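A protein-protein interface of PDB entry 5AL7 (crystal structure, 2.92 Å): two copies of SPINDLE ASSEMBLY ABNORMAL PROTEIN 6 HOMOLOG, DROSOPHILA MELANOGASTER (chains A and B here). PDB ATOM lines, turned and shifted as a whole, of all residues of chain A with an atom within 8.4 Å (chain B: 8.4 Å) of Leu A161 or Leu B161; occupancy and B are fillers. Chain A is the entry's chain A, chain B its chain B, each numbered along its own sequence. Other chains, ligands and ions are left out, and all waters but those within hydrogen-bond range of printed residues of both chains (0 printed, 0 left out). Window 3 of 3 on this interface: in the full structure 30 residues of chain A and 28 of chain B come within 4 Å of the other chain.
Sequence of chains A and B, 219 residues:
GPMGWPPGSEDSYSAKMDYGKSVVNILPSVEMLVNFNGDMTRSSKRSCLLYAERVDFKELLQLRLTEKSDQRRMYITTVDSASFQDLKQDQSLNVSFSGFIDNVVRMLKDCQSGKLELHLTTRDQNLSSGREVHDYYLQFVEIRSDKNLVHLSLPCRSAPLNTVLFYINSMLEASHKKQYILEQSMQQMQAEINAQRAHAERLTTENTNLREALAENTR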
ATOM      1  N   SER A  12     -12.865 -28.627   2.649  1.00  0.00           N
ATOM      2  CA  SER A  12     -14.316 -28.496   2.569  1.00  0.00           C
ATOM      3  C   SER A  12     -14.790 -27.329   3.432  1.00  0.00           C
ATOM      4  O   SER A  12     -14.005 -26.726   4.168  1.00  0.00           O
ATOM      5  CB  SER A  12     -15.008 -29.799   2.990  1.00  0.00           C
ATOM      6  OG  SER A  12     -16.407 -29.747   2.751  1.00  0.00           O
ATOM      7  N   TYR A  13     -16.078 -27.022   3.341  1.00  0.00           N
ATOM      8  CA  TYR A  13     -16.643 -25.881   4.048  1.00  0.00           C
ATOM      9  C   TYR A  13     -17.498 -26.324   5.225  1.00  0.00           C
ATOM     10  O   TYR A  13     -18.268 -27.281   5.123  1.00  0.00           O
ATOM     11  CB  TYR A  13     -17.483 -25.036   3.081  1.00  0.00           C
ATOM     12  CG  TYR A  13     -18.462 -24.087   3.744  1.00  0.00           C
ATOM     13  CD1 TYR A  13     -18.042 -22.861   4.241  1.00  0.00           C
ATOM     14  CD2 TYR A  13     -19.810 -24.415   3.862  1.00  0.00           C
ATOM     15  CE1 TYR A  13     -18.931 -21.991   4.843  1.00  0.00           C
ATOM     16  CE2 TYR A  13     -20.707 -23.551   4.464  1.00  0.00           C
ATOM     17  CZ  TYR A  13     -20.261 -22.340   4.952  1.00  0.00           C
ATOM     18  OH  TYR A  13     -21.143 -21.470   5.553  1.00  0.00           O
ATOM     19  N   SER A  14     -17.374 -25.606   6.336  1.00  0.00           N
ATOM     20  CA  SER A  14     -18.234 -25.830   7.492  1.00  0.00           C
ATOM     21  C   SER A  14     -18.262 -24.623   8.382  1.00  0.00           C
ATOM     22  O   SER A  14     -17.259 -23.937   8.557  1.00  0.00           O
ATOM     23  CB  SER A  14     -17.789 -27.032   8.325  1.00  0.00           C
ATOM     24  OG  SER A  14     -18.688 -27.263   9.405  1.00  0.00           O
ATOM     25  N   LYS A  16     -18.046 -22.251  11.285  1.00  0.00           N
ATOM     26  CA  LYS A  16     -17.207 -22.080  12.457  1.00  0.00           C
ATOM     27  C   LYS A  16     -17.865 -21.047  13.341  1.00  0.00           C
ATOM     28  O   LYS A  16     -18.319 -20.018  12.855  1.00  0.00           O
ATOM     29  CB  LYS A  16     -15.802 -21.623  12.070  1.00  0.00           C
ATOM     30  CG  LYS A  16     -15.072 -22.581  11.180  1.00  0.00           C
ATOM     31  CD  LYS A  16     -14.094 -21.840  10.298  1.00  0.00           C
ATOM     32  CE  LYS A  16     -13.678 -22.730   9.139  1.00  0.00           C
ATOM     33  NZ  LYS A  16     -14.800 -22.957   8.169  1.00  0.00           N
ATOM     34  N   ARG A  72      -9.868 -35.080  17.319  1.00  0.00           N
ATOM     35  CA  ARG A  72      -9.830 -34.828  15.881  1.00  0.00           C
ATOM     36  C   ARG A  72     -11.038 -35.454  15.197  1.00  0.00           C
ATOM     37  O   ARG A  72     -11.386 -35.095  14.071  1.00  0.00           O
ATOM     38  CB  ARG A  72      -8.551 -35.390  15.274  1.00  0.00           C
ATOM     39  CG  ARG A  72      -7.294 -34.683  15.731  1.00  0.00           C
ATOM     40  CD  ARG A  72      -6.102 -35.273  15.046  1.00  0.00           C
ATOM     41  NE  ARG A  72      -5.827 -36.633  15.491  1.00  0.00           N
ATOM     42  CZ  ARG A  72      -4.927 -37.416  14.917  1.00  0.00           C
ATOM     43  NH1 ARG A  72      -4.242 -36.960  13.877  1.00  0.00           N
ATOM     44  NH2 ARG A  72      -4.715 -38.648  15.372  1.00  0.00           N
ATOM     45  N   MET A  74     -14.380 -35.280  14.919  1.00  0.00           N
ATOM     46  CA  MET A  74     -15.396 -34.280  15.217  1.00  0.00           C
ATOM     47  C   MET A  74     -16.623 -34.339  14.321  1.00  0.00           C
ATOM     48  O   MET A  74     -16.517 -34.450  13.098  1.00  0.00           O
ATOM     49  CB  MET A  74     -14.772 -32.887  15.139  1.00  0.00           C
ATOM     50  CG  MET A  74     -15.547 -31.802  15.851  1.00  0.00           C
ATOM     51  SD  MET A  74     -14.609 -30.277  15.817  1.00  0.00           S
ATOM     52  CE  MET A  74     -13.343 -30.648  17.025  1.00  0.00           C
ATOM     53  N   ARG A 157     -23.002 -33.575  10.616  1.00  0.00           N
ATOM     54  CA  ARG A 157     -21.985 -33.586   9.583  1.00  0.00           C
ATOM     55  C   ARG A 157     -20.644 -34.032  10.134  1.00  0.00           C
ATOM     56  O   ARG A 157     -20.339 -33.830  11.314  1.00  0.00           O
ATOM     57  CB  ARG A 157     -21.884 -32.183   8.980  1.00  0.00           C
ATOM     58  CG  ARG A 157     -21.040 -32.053   7.742  1.00  0.00           C
ATOM     59  CD  ARG A 157     -20.312 -30.714   7.751  1.00  0.00           C
ATOM     60  NE  ARG A 157     -19.949 -30.246   6.412  1.00  0.00           N
ATOM     61  CZ  ARG A 157     -18.879 -30.666   5.743  1.00  0.00           C
ATOM     62  NH1 ARG A 157     -18.078 -31.580   6.277  1.00  0.00           N
ATOM     63  NH2 ARG A 157     -18.619 -30.185   4.535  1.00  0.00           N
ATOM     64  N   SER A 158     -19.844 -34.669   9.294  1.00  0.00           N
ATOM     65  CA  SER A 158     -18.477 -34.987   9.689  1.00  0.00           C
ATOM     66  C   SER A 158     -17.583 -33.783   9.407  1.00  0.00           C
ATOM     67  O   SER A 158     -17.397 -33.402   8.249  1.00  0.00           O
ATOM     68  CB  SER A 158     -17.972 -36.212   8.963  1.00  0.00           C
ATOM     69  OG  SER A 158     -16.820 -36.676   9.624  1.00  0.00           O
ATOM     70  N   ALA A 159     -17.081 -33.151  10.465  1.00  0.00           N
ATOM     71  CA  ALA A 159     -16.344 -31.895  10.332  1.00  0.00           C
ATOM     72  C   ALA A 159     -15.115 -32.001   9.424  1.00  0.00           C
ATOM     73  O   ALA A 159     -14.279 -32.905   9.575  1.00  0.00           O
ATOM     74  CB  ALA A 159     -15.936 -31.392  11.699  1.00  0.00           C
ATOM     75  N   PRO A 160     -15.007 -31.075   8.464  1.00  0.00           N
ATOM     76  CA  PRO A 160     -13.854 -31.000   7.560  1.00  0.00           C
ATOM     77  C   PRO A 160     -12.605 -30.471   8.266  1.00  0.00           C
ATOM     78  O   PRO A 160     -12.704 -29.752   9.270  1.00  0.00           O
ATOM     79  CB  PRO A 160     -14.328 -30.034   6.480  1.00  0.00           C
ATOM     80  CG  PRO A 160     -15.322 -29.178   7.157  1.00  0.00           C
ATOM     81  CD  PRO A 160     -16.006 -30.035   8.178  1.00  0.00           C
ATOM     82  N   LEU A 161     -11.441 -30.827   7.732  1.00  0.00           N
ATOM     83  CA  LEU A 161     -10.160 -30.554   8.390  1.00  0.00           C
ATOM     84  C   LEU A 161      -9.959 -29.118   8.816  1.00  0.00           C
ATOM     85  O   LEU A 161      -9.502 -28.864   9.927  1.00  0.00           O
ATOM     86  CB  LEU A 161      -9.004 -30.970   7.484  1.00  0.00           C
ATOM     87  CG  LEU A 161      -8.433 -32.317   7.898  1.00  0.00           C
ATOM     88  CD1 LEU A 161      -9.485 -33.421   7.699  1.00  0.00           C
ATOM     89  CD2 LEU A 161      -7.166 -32.602   7.112  1.00  0.00           C
ATOM     90  N   ASN A 162     -10.331 -28.175   7.963  1.00  0.00           N
ATOM     91  CA  ASN A 162     -10.110 -26.786   8.316  1.00  0.00           C
ATOM     92  C   ASN A 162     -10.807 -26.420   9.620  1.00  0.00           C
ATOM     93  O   ASN A 162     -10.188 -25.855  10.534  1.00  0.00           O
ATOM     94  CB  ASN A 162     -10.577 -25.859   7.205  1.00  0.00           C
ATOM     95  CG  ASN A 162      -9.979 -24.475   7.337  1.00  0.00           C
ATOM     96  OD1 ASN A 162     -10.685 -23.496   7.599  1.00  0.00           O
ATOM     97  ND2 ASN A 162      -8.654 -24.392   7.195  1.00  0.00           N
ATOM     98  N   THR A 163     -12.072 -26.817   9.727  1.00  0.00           N
ATOM     99  CA  THR A 163     -12.889 -26.506  10.892  1.00  0.00           C
ATOM    100  C   THR A 163     -12.364 -27.190  12.146  1.00  0.00           C
ATOM    101  O   THR A 163     -12.262 -26.576  13.220  1.00  0.00           O
ATOM    102  CB  THR A 163     -14.333 -26.946  10.673  1.00  0.00           C
ATOM    103  OG1 THR A 163     -14.763 -26.546   9.364  1.00  0.00           O
ATOM    104  CG2 THR A 163     -15.238 -26.365  11.749  1.00  0.00           C
ATOM    105  N   VAL A 164     -12.023 -28.466  11.998  1.00  0.00           N
ATOM    106  CA  VAL A 164     -11.476 -29.236  13.102  1.00  0.00           C
ATOM    107  C   VAL A 164     -10.217 -28.592  13.644  1.00  0.00           C
ATOM    108  O   VAL A 164     -10.055 -28.430  14.855  1.00  0.00           O
ATOM    109  CB  VAL A 164     -11.150 -30.669  12.679  1.00  0.00           C
ATOM    110  CG1 VAL A 164     -10.547 -31.429  13.834  1.00  0.00           C
ATOM    111  CG2 VAL A 164     -12.406 -31.364  12.204  1.00  0.00           C
ATOM    112  N   LEU A 165      -9.345 -28.199  12.722  1.00  0.00           N
ATOM    113  CA  LEU A 165      -8.079 -27.572  13.061  1.00  0.00           C
ATOM    114  C   LEU A 165      -8.324 -26.265  13.788  1.00  0.00           C
ATOM    115  O   LEU A 165      -7.596 -25.929  14.721  1.00  0.00           O
ATOM    116  CB  LEU A 165      -7.247 -27.373  11.796  1.00  0.00           C
ATOM    117  CG  LEU A 165      -5.821 -26.852  11.942  1.00  0.00           C
ATOM    118  CD1 LEU A 165      -5.127 -27.647  13.028  1.00  0.00           C
ATOM    119  CD2 LEU A 165      -5.091 -27.010  10.613  1.00  0.00           C
ATOM    120  N   PHE A 166      -9.374 -25.555  13.372  1.00  0.00           N
ATOM    121  CA  PHE A 166      -9.784 -24.326  14.037  1.00  0.00           C
ATOM    122  C   PHE A 166     -10.150 -24.580  15.503  1.00  0.00           C
ATOM    123  O   PHE A 166      -9.675 -23.883  16.414  1.00  0.00           O
ATOM    124  CB  PHE A 166     -10.966 -23.692  13.306  1.00  0.00           C
ATOM    125  CG  PHE A 166     -11.615 -22.563  14.063  1.00  0.00           C
ATOM    126  CD1 PHE A 166     -11.053 -21.291  14.046  1.00  0.00           C
ATOM    127  CD2 PHE A 166     -12.771 -22.776  14.811  1.00  0.00           C
ATOM    128  CE1 PHE A 166     -11.641 -20.254  14.750  1.00  0.00           C
ATOM    129  CE2 PHE A 166     -13.358 -21.748  15.514  1.00  0.00           C
ATOM    130  CZ  PHE A 166     -12.794 -20.483  15.486  1.00  0.00           C
ATOM    131  N   TYR A 167     -11.022 -25.555  15.740  1.00  0.00           N
ATOM    132  CA  TYR A 167     -11.452 -25.811  17.113  1.00  0.00           C
ATOM    133  C   TYR A 167     -10.349 -26.415  18.000  1.00  0.00           C
ATOM    134  O   TYR A 167     -10.212 -26.059  19.172  1.00  0.00           O
ATOM    135  CB  TYR A 167     -12.697 -26.690  17.114  1.00  0.00           C
ATOM    136  CG  TYR A 167     -13.931 -25.943  16.667  1.00  0.00           C
ATOM    137  CD1 TYR A 167     -14.447 -24.891  17.425  1.00  0.00           C
ATOM    138  CD2 TYR A 167     -14.585 -26.290  15.493  1.00  0.00           C
ATOM    139  CE1 TYR A 167     -15.570 -24.201  17.019  1.00  0.00           C
ATOM    140  CE2 TYR A 167     -15.707 -25.607  15.082  1.00  0.00           C
ATOM    141  CZ  TYR A 167     -16.200 -24.564  15.848  1.00  0.00           C
ATOM    142  OH  TYR A 167     -17.324 -23.889  15.421  1.00  0.00           O
ATOM    143  N   ILE A 168      -9.551 -27.318  17.454  1.00  0.00           N
ATOM    144  CA  ILE A 168      -8.486 -27.910  18.254  1.00  0.00           C
ATOM    145  C   ILE A 168      -7.379 -26.879  18.541  1.00  0.00           C
ATOM    146  O   ILE A 168      -6.827 -26.842  19.649  1.00  0.00           O
ATOM    147  CB  ILE A 168      -7.923 -29.190  17.566  1.00  0.00           C
ATOM    148  CG1 ILE A 168      -8.858 -30.363  17.843  1.00  0.00           C
ATOM    149  CG2 ILE A 168      -6.554 -29.542  18.076  1.00  0.00           C
ATOM    150  CD1 ILE A 168      -8.836 -31.391  16.798  1.00  0.00           C
ATOM    151  N   SER B  12      -2.956 -34.782   1.069  1.00  0.00           N
ATOM    152  CA  SER B  12      -1.755 -34.030   1.416  1.00  0.00           C
ATOM    153  C   SER B  12      -0.868 -34.798   2.401  1.00  0.00           C
ATOM    154  O   SER B  12      -1.258 -35.049   3.543  1.00  0.00           O
ATOM    155  CB  SER B  12      -2.135 -32.669   1.998  1.00  0.00           C
ATOM    156  OG  SER B  12      -2.851 -32.813   3.213  1.00  0.00           O
ATOM    157  N   TYR B  13       0.336 -35.145   1.952  1.00  0.00           N
ATOM    158  CA  TYR B  13       1.264 -35.953   2.742  1.00  0.00           C
ATOM    159  C   TYR B  13       2.471 -35.177   3.262  1.00  0.00           C
ATOM    160  O   TYR B  13       3.038 -34.334   2.567  1.00  0.00           O
ATOM    161  CB  TYR B  13       1.756 -37.150   1.915  1.00  0.00           C
ATOM    162  CG  TYR B  13       3.024 -37.801   2.446  1.00  0.00           C
ATOM    163  CD1 TYR B  13       2.980 -38.705   3.502  1.00  0.00           C
ATOM    164  CD2 TYR B  13       4.266 -37.509   1.885  1.00  0.00           C
ATOM    165  CE1 TYR B  13       4.137 -39.296   3.986  1.00  0.00           C
ATOM    166  CE2 TYR B  13       5.425 -38.095   2.364  1.00  0.00           C
ATOM    167  CZ  TYR B  13       5.354 -38.988   3.414  1.00  0.00           C
ATOM    168  OH  TYR B  13       6.504 -39.572   3.891  1.00  0.00           O
ATOM    169  N   SER B  14       2.858 -35.497   4.492  1.00  0.00           N
ATOM    170  CA  SER B  14       4.077 -34.990   5.113  1.00  0.00           C
ATOM    171  C   SER B  14       4.507 -35.896   6.238  1.00  0.00           C
ATOM    172  O   SER B  14       3.678 -36.511   6.911  1.00  0.00           O
ATOM    173  CB  SER B  14       3.917 -33.578   5.666  1.00  0.00           C
ATOM    174  OG  SER B  14       5.146 -33.135   6.224  1.00  0.00           O
ATOM    175  N   LYS B  16       5.420 -37.276   9.610  1.00  0.00           N
ATOM    176  CA  LYS B  16       5.031 -37.037  10.991  1.00  0.00           C
ATOM    177  C   LYS B  16       5.991 -37.791  11.896  1.00  0.00           C
ATOM    178  O   LYS B  16       6.302 -38.949  11.630  1.00  0.00           O
ATOM    179  CB  LYS B  16       3.601 -37.511  11.246  1.00  0.00           C
ATOM    180  CG  LYS B  16       2.572 -36.843  10.376  1.00  0.00           C
ATOM    181  CD  LYS B  16       1.384 -37.769  10.146  1.00  0.00           C
ATOM    182  CE  LYS B  16       0.572 -37.293   8.950  1.00  0.00           C
ATOM    183  NZ  LYS B  16       1.317 -37.500   7.663  1.00  0.00           N
ATOM    184  N   ARG B  72      -1.016 -22.840  13.844  1.00  0.00           N
ATOM    185  CA  ARG B  72      -1.517 -23.509  12.642  1.00  0.00           C
ATOM    186  C   ARG B  72      -0.625 -23.196  11.447  1.00  0.00           C
ATOM    187  O   ARG B  72      -0.644 -23.911  10.440  1.00  0.00           O
ATOM    188  CB  ARG B  72      -2.954 -23.080  12.337  1.00  0.00           C
ATOM    189  CG  ARG B  72      -3.989 -23.546  13.343  1.00  0.00           C
ATOM    190  CD  ARG B  72      -5.385 -23.101  12.940  1.00  0.00           C
ATOM    191  NE  ARG B  72      -5.562 -21.654  13.053  1.00  0.00           N
ATOM    192  CZ  ARG B  72      -6.635 -20.993  12.628  1.00  0.00           C
ATOM    193  NH1 ARG B  72      -7.639 -21.645  12.055  1.00  0.00           N
ATOM    194  NH2 ARG B  72      -6.708 -19.677  12.777  1.00  0.00           N
ATOM    195  N   MET B  74       2.515 -23.587  10.211  1.00  0.00           N
ATOM    196  CA  MET B  74       3.615 -24.500  10.475  1.00  0.00           C
ATOM    197  C   MET B  74       4.484 -24.755   9.239  1.00  0.00           C
ATOM    198  O   MET B  74       3.987 -24.995   8.132  1.00  0.00           O
ATOM    199  CB  MET B  74       3.057 -25.819  11.021  1.00  0.00           C
ATOM    200  CG  MET B  74       4.048 -26.676  11.781  1.00  0.00           C
ATOM    201  SD  MET B  74       3.311 -28.152  12.505  1.00  0.00           S
ATOM    202  CE  MET B  74       2.390 -27.453  13.876  1.00  0.00           C
ATOM    203  N   ARG B 157       9.324 -26.971   4.084  1.00  0.00           N
ATOM    204  CA  ARG B 157       8.036 -27.221   3.455  1.00  0.00           C
ATOM    205  C   ARG B 157       6.934 -26.553   4.260  1.00  0.00           C
ATOM    206  O   ARG B 157       7.042 -26.413   5.482  1.00  0.00           O
ATOM    207  CB  ARG B 157       7.792 -28.724   3.354  1.00  0.00           C
ATOM    208  CG  ARG B 157       6.608 -29.129   2.539  1.00  0.00           C
ATOM    209  CD  ARG B 157       5.936 -30.333   3.185  1.00  0.00           C
ATOM    210  NE  ARG B 157       5.160 -31.137   2.239  1.00  0.00           N
ATOM    211  CZ  ARG B 157       3.931 -30.829   1.835  1.00  0.00           C
ATOM    212  NH1 ARG B 157       3.346 -29.721   2.275  1.00  0.00           N
ATOM    213  NH2 ARG B 157       3.296 -31.615   0.977  1.00  0.00           N
ATOM    214  N   SER B 158       5.880 -26.123   3.586  1.00  0.00           N
ATOM    215  CA  SER B 158       4.725 -25.592   4.296  1.00  0.00           C
ATOM    216  C   SER B 158       3.811 -26.744   4.713  1.00  0.00           C
ATOM    217  O   SER B 158       3.214 -27.407   3.865  1.00  0.00           O
ATOM    218  CB  SER B 158       3.976 -24.582   3.437  1.00  0.00           C
ATOM    219  OG  SER B 158       3.091 -23.848   4.254  1.00  0.00           O
ATOM    220  N   ALA B 159       3.722 -26.993   6.014  1.00  0.00           N
ATOM    221  CA  ALA B 159       3.028 -28.176   6.519  1.00  0.00           C
ATOM    222  C   ALA B 159       1.568 -28.269   6.067  1.00  0.00           C
ATOM    223  O   ALA B 159       0.805 -27.311   6.182  1.00  0.00           O
ATOM    224  CB  ALA B 159       3.106 -28.214   8.042  1.00  0.00           C
ATOM    225  N   PRO B 160       1.187 -29.430   5.519  1.00  0.00           N
ATOM    226  CA  PRO B 160      -0.189 -29.713   5.101  1.00  0.00           C
ATOM    227  C   PRO B 160      -1.116 -29.959   6.294  1.00  0.00           C
ATOM    228  O   PRO B 160      -0.660 -30.353   7.378  1.00  0.00           O
ATOM    229  CB  PRO B 160      -0.036 -30.964   4.244  1.00  0.00           C
ATOM    230  CG  PRO B 160       1.167 -31.628   4.767  1.00  0.00           C
ATOM    231  CD  PRO B 160       2.094 -30.551   5.225  1.00  0.00           C
ATOM    232  N   LEU B 161      -2.408 -29.725   6.085  1.00  0.00           N
ATOM    233  CA  LEU B 161      -3.387 -29.736   7.174  1.00  0.00           C
ATOM    234  C   LEU B 161      -3.358 -30.970   8.034  1.00  0.00           C
ATOM    235  O   LEU B 161      -3.455 -30.887   9.258  1.00  0.00           O
ATOM    236  CB  LEU B 161      -4.799 -29.556   6.628  1.00  0.00           C
ATOM    237  CG  LEU B 161      -5.238 -28.125   6.834  1.00  0.00           C
ATOM    238  CD1 LEU B 161      -4.348 -27.193   5.996  1.00  0.00           C
ATOM    239  CD2 LEU B 161      -6.698 -28.004   6.454  1.00  0.00           C
ATOM    240  N   ASN B 162      -3.205 -32.121   7.403  1.00  0.00           N
ATOM    241  CA  ASN B 162      -3.249 -33.343   8.165  1.00  0.00           C
ATOM    242  C   ASN B 162      -2.182 -33.353   9.247  1.00  0.00           C
ATOM    243  O   ASN B 162      -2.458 -33.621  10.425  1.00  0.00           O
ATOM    244  CB  ASN B 162      -3.084 -34.543   7.257  1.00  0.00           C
ATOM    245  CG  ASN B 162      -3.583 -35.798   7.904  1.00  0.00           C
ATOM    246  OD1 ASN B 162      -4.777 -35.909   8.206  1.00  0.00           O
ATOM    247  ND2 ASN B 162      -2.684 -36.746   8.152  1.00  0.00           N
ATOM    248  N   THR B 163      -0.973 -32.989   8.848  1.00  0.00           N
ATOM    249  CA  THR B 163       0.162 -32.975   9.748  1.00  0.00           C
ATOM    250  C   THR B 163       0.013 -31.932  10.843  1.00  0.00           C
ATOM    251  O   THR B 163       0.236 -32.219  12.031  1.00  0.00           O
ATOM    252  CB  THR B 163       1.437 -32.708   8.971  1.00  0.00           C
ATOM    253  OG1 THR B 163       1.477 -33.589   7.843  1.00  0.00           O
ATOM    254  CG2 THR B 163       2.672 -32.926   9.849  1.00  0.00           C
ATOM    255  N   VAL B 164      -0.398 -30.733  10.445  1.00  0.00           N
ATOM    256  CA  VAL B 164      -0.597 -29.662  11.399  1.00  0.00           C
ATOM    257  C   VAL B 164      -1.604 -30.088  12.465  1.00  0.00           C
ATOM    258  O   VAL B 164      -1.370 -29.917  13.661  1.00  0.00           O
ATOM    259  CB  VAL B 164      -1.086 -28.389  10.705  1.00  0.00           C
ATOM    260  CG1 VAL B 164      -1.303 -27.303  11.714  1.00  0.00           C
ATOM    261  CG2 VAL B 164      -0.073 -27.942   9.681  1.00  0.00           C
ATOM    262  N   LEU B 165      -2.705 -30.686  12.022  1.00  0.00           N
ATOM    263  CA  LEU B 165      -3.750 -31.155  12.924  1.00  0.00           C
ATOM    264  C   LEU B 165      -3.221 -32.233  13.858  1.00  0.00           C
ATOM    265  O   LEU B 165      -3.594 -32.280  15.031  1.00  0.00           O
ATOM    266  CB  LEU B 165      -4.944 -31.654  12.122  1.00  0.00           C
ATOM    267  CG  LEU B 165      -6.198 -32.066  12.889  1.00  0.00           C
ATOM    268  CD1 LEU B 165      -6.552 -31.000  13.912  1.00  0.00           C
ATOM    269  CD2 LEU B 165      -7.331 -32.235  11.896  1.00  0.00           C
ATOM    270  N   PHE B 166      -2.331 -33.078  13.343  1.00  0.00           N
ATOM    271  CA  PHE B 166      -1.686 -34.087  14.179  1.00  0.00           C
ATOM    272  C   PHE B 166      -0.902 -33.432  15.322  1.00  0.00           C
ATOM    273  O   PHE B 166      -1.086 -33.779  16.502  1.00  0.00           O
ATOM    274  CB  PHE B 166      -0.761 -34.972  13.336  1.00  0.00           C
ATOM    275  CG  PHE B 166       0.174 -35.835  14.149  1.00  0.00           C
ATOM    276  CD1 PHE B 166      -0.275 -37.002  14.741  1.00  0.00           C
ATOM    277  CD2 PHE B 166       1.503 -35.484  14.307  1.00  0.00           C
ATOM    278  CE1 PHE B 166       0.579 -37.786  15.483  1.00  0.00           C
ATOM    279  CE2 PHE B 166       2.353 -36.269  15.051  1.00  0.00           C
ATOM    280  CZ  PHE B 166       1.894 -37.420  15.636  1.00  0.00           C
ATOM    281  N   TYR B 167      -0.029 -32.488  14.981  1.00  0.00           N
ATOM    282  CA  TYR B 167       0.809 -31.864  16.003  1.00  0.00           C
ATOM    283  C   TYR B 167       0.028 -30.966  16.971  1.00  0.00           C
ATOM    284  O   TYR B 167       0.310 -30.926  18.171  1.00  0.00           O
ATOM    285  CB  TYR B 167       1.948 -31.076  15.349  1.00  0.00           C
ATOM    286  CG  TYR B 167       3.020 -31.965  14.765  1.00  0.00           C
ATOM    287  CD1 TYR B 167       3.828 -32.751  15.587  1.00  0.00           C
ATOM    288  CD2 TYR B 167       3.219 -32.031  13.386  1.00  0.00           C
ATOM    289  CE1 TYR B 167       4.802 -33.574  15.050  1.00  0.00           C
ATOM    290  CE2 TYR B 167       4.190 -32.848  12.848  1.00  0.00           C
ATOM    291  CZ  TYR B 167       4.976 -33.616  13.683  1.00  0.00           C
ATOM    292  OH  TYR B 167       5.936 -34.423  13.125  1.00  0.00           O
ATOM    293  N   ILE B 168      -0.946 -30.229  16.468  1.00  0.00           N
ATOM    294  CA  ILE B 168      -1.701 -29.355  17.358  1.00  0.00           C
ATOM    295  C   ILE B 168      -2.592 -30.178  18.284  1.00  0.00           C
ATOM    296  O   ILE B 168      -2.707 -29.864  19.476  1.00  0.00           O
ATOM    297  CB  ILE B 168      -2.498 -28.309  16.559  1.00  0.00           C
ATOM    298  CG1 ILE B 168      -1.552 -27.167  16.190  1.00  0.00           C
ATOM    299  CG2 ILE B 168      -3.655 -27.757  17.363  1.00  0.00           C
ATOM    300  CD1 ILE B 168      -1.919 -26.469  14.950  1.00  0.00           C
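Arg A72 touches Leu B165, and with the chains exchanged Leu A165 touches Arg B72.
Asn A162 touches Leu B161, but with the chains exchanged Leu A161 does not touch Asn B162 (4.001 Å).
Val A164 touches Leu B165, and with the chains exchanged Leu A165 touches Val B164.
Leu A165 touches Ile B168, and with the chains exchanged Ile A168 touches Leu B165.
Positions printed for both chains: 12, 13, 14, 16, 72, 74, 157, 158, 159, 160, 161, 162, 163, 164, 165, 166, 167 and 168.
Of the 13 pairs that touch across the chains among the printed residues, 11 have their exchanged pair printed and touching as well.
Of the printed residues of chain B, Leu A161 touches Leu B161.
Of chain A, only Leu A161 (3.9 Å), Asn A162 (3.9 Å) and Leu A165 (3.9 Å) come within 4 Å of Leu B161.
Of the printed residues of chain A, Ile B168 touches Leu A165 (3.9 Å) and Ile A168 (3.5 Å).
Printed residues of chain A within 4 Å of Val B164: Leu A165 (3.96 Å).
Of the printed residues of chain A, Leu B165 touches Arg A72, Val A164, Leu A165 and Ile A168.
Printed residues of chain B within 4 Å of Phe A166: Arg B72 (3.96 Å).
Of the printed residues of chain A, Phe B166 touches Arg A72 (3.9 Å).
Tyr B167 touches none of the printed residues of chain A.
The nearest printed residue of chain B that does not touch Leu A161 is Asn B162 (4.001 Å).
Among the printed residues, pairs that only touch across the chains: Arg A72 with Leu B165, Arg A72 with Phe B166, Leu A161 with Leu B161, Asn A162 with Leu B161, Val A164 with Leu B165, Leu A165 with Arg B72, Leu A165 with Leu B161, Leu A165 with Val B164, Leu A165 with Leu B165, Leu A165 with Ile B168, Phe A166 with Arg B72, Ile A168 with Leu B165 and Ile A168 with Ile B168.
Printed residues of chain A that touch a printed residue of chain B: Arg A72, Leu A161, Asn A162, Val A164, Leu A165, Phe A166 and Ile A168.
Hydrophobic or aromatic side chains of chain A within 4 Å of the printed part of chain B: Leu A161, Val A164, Leu A165, Phe A166 and Ile A168.
Among the printed residues, 13 pairs touch across the chains.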
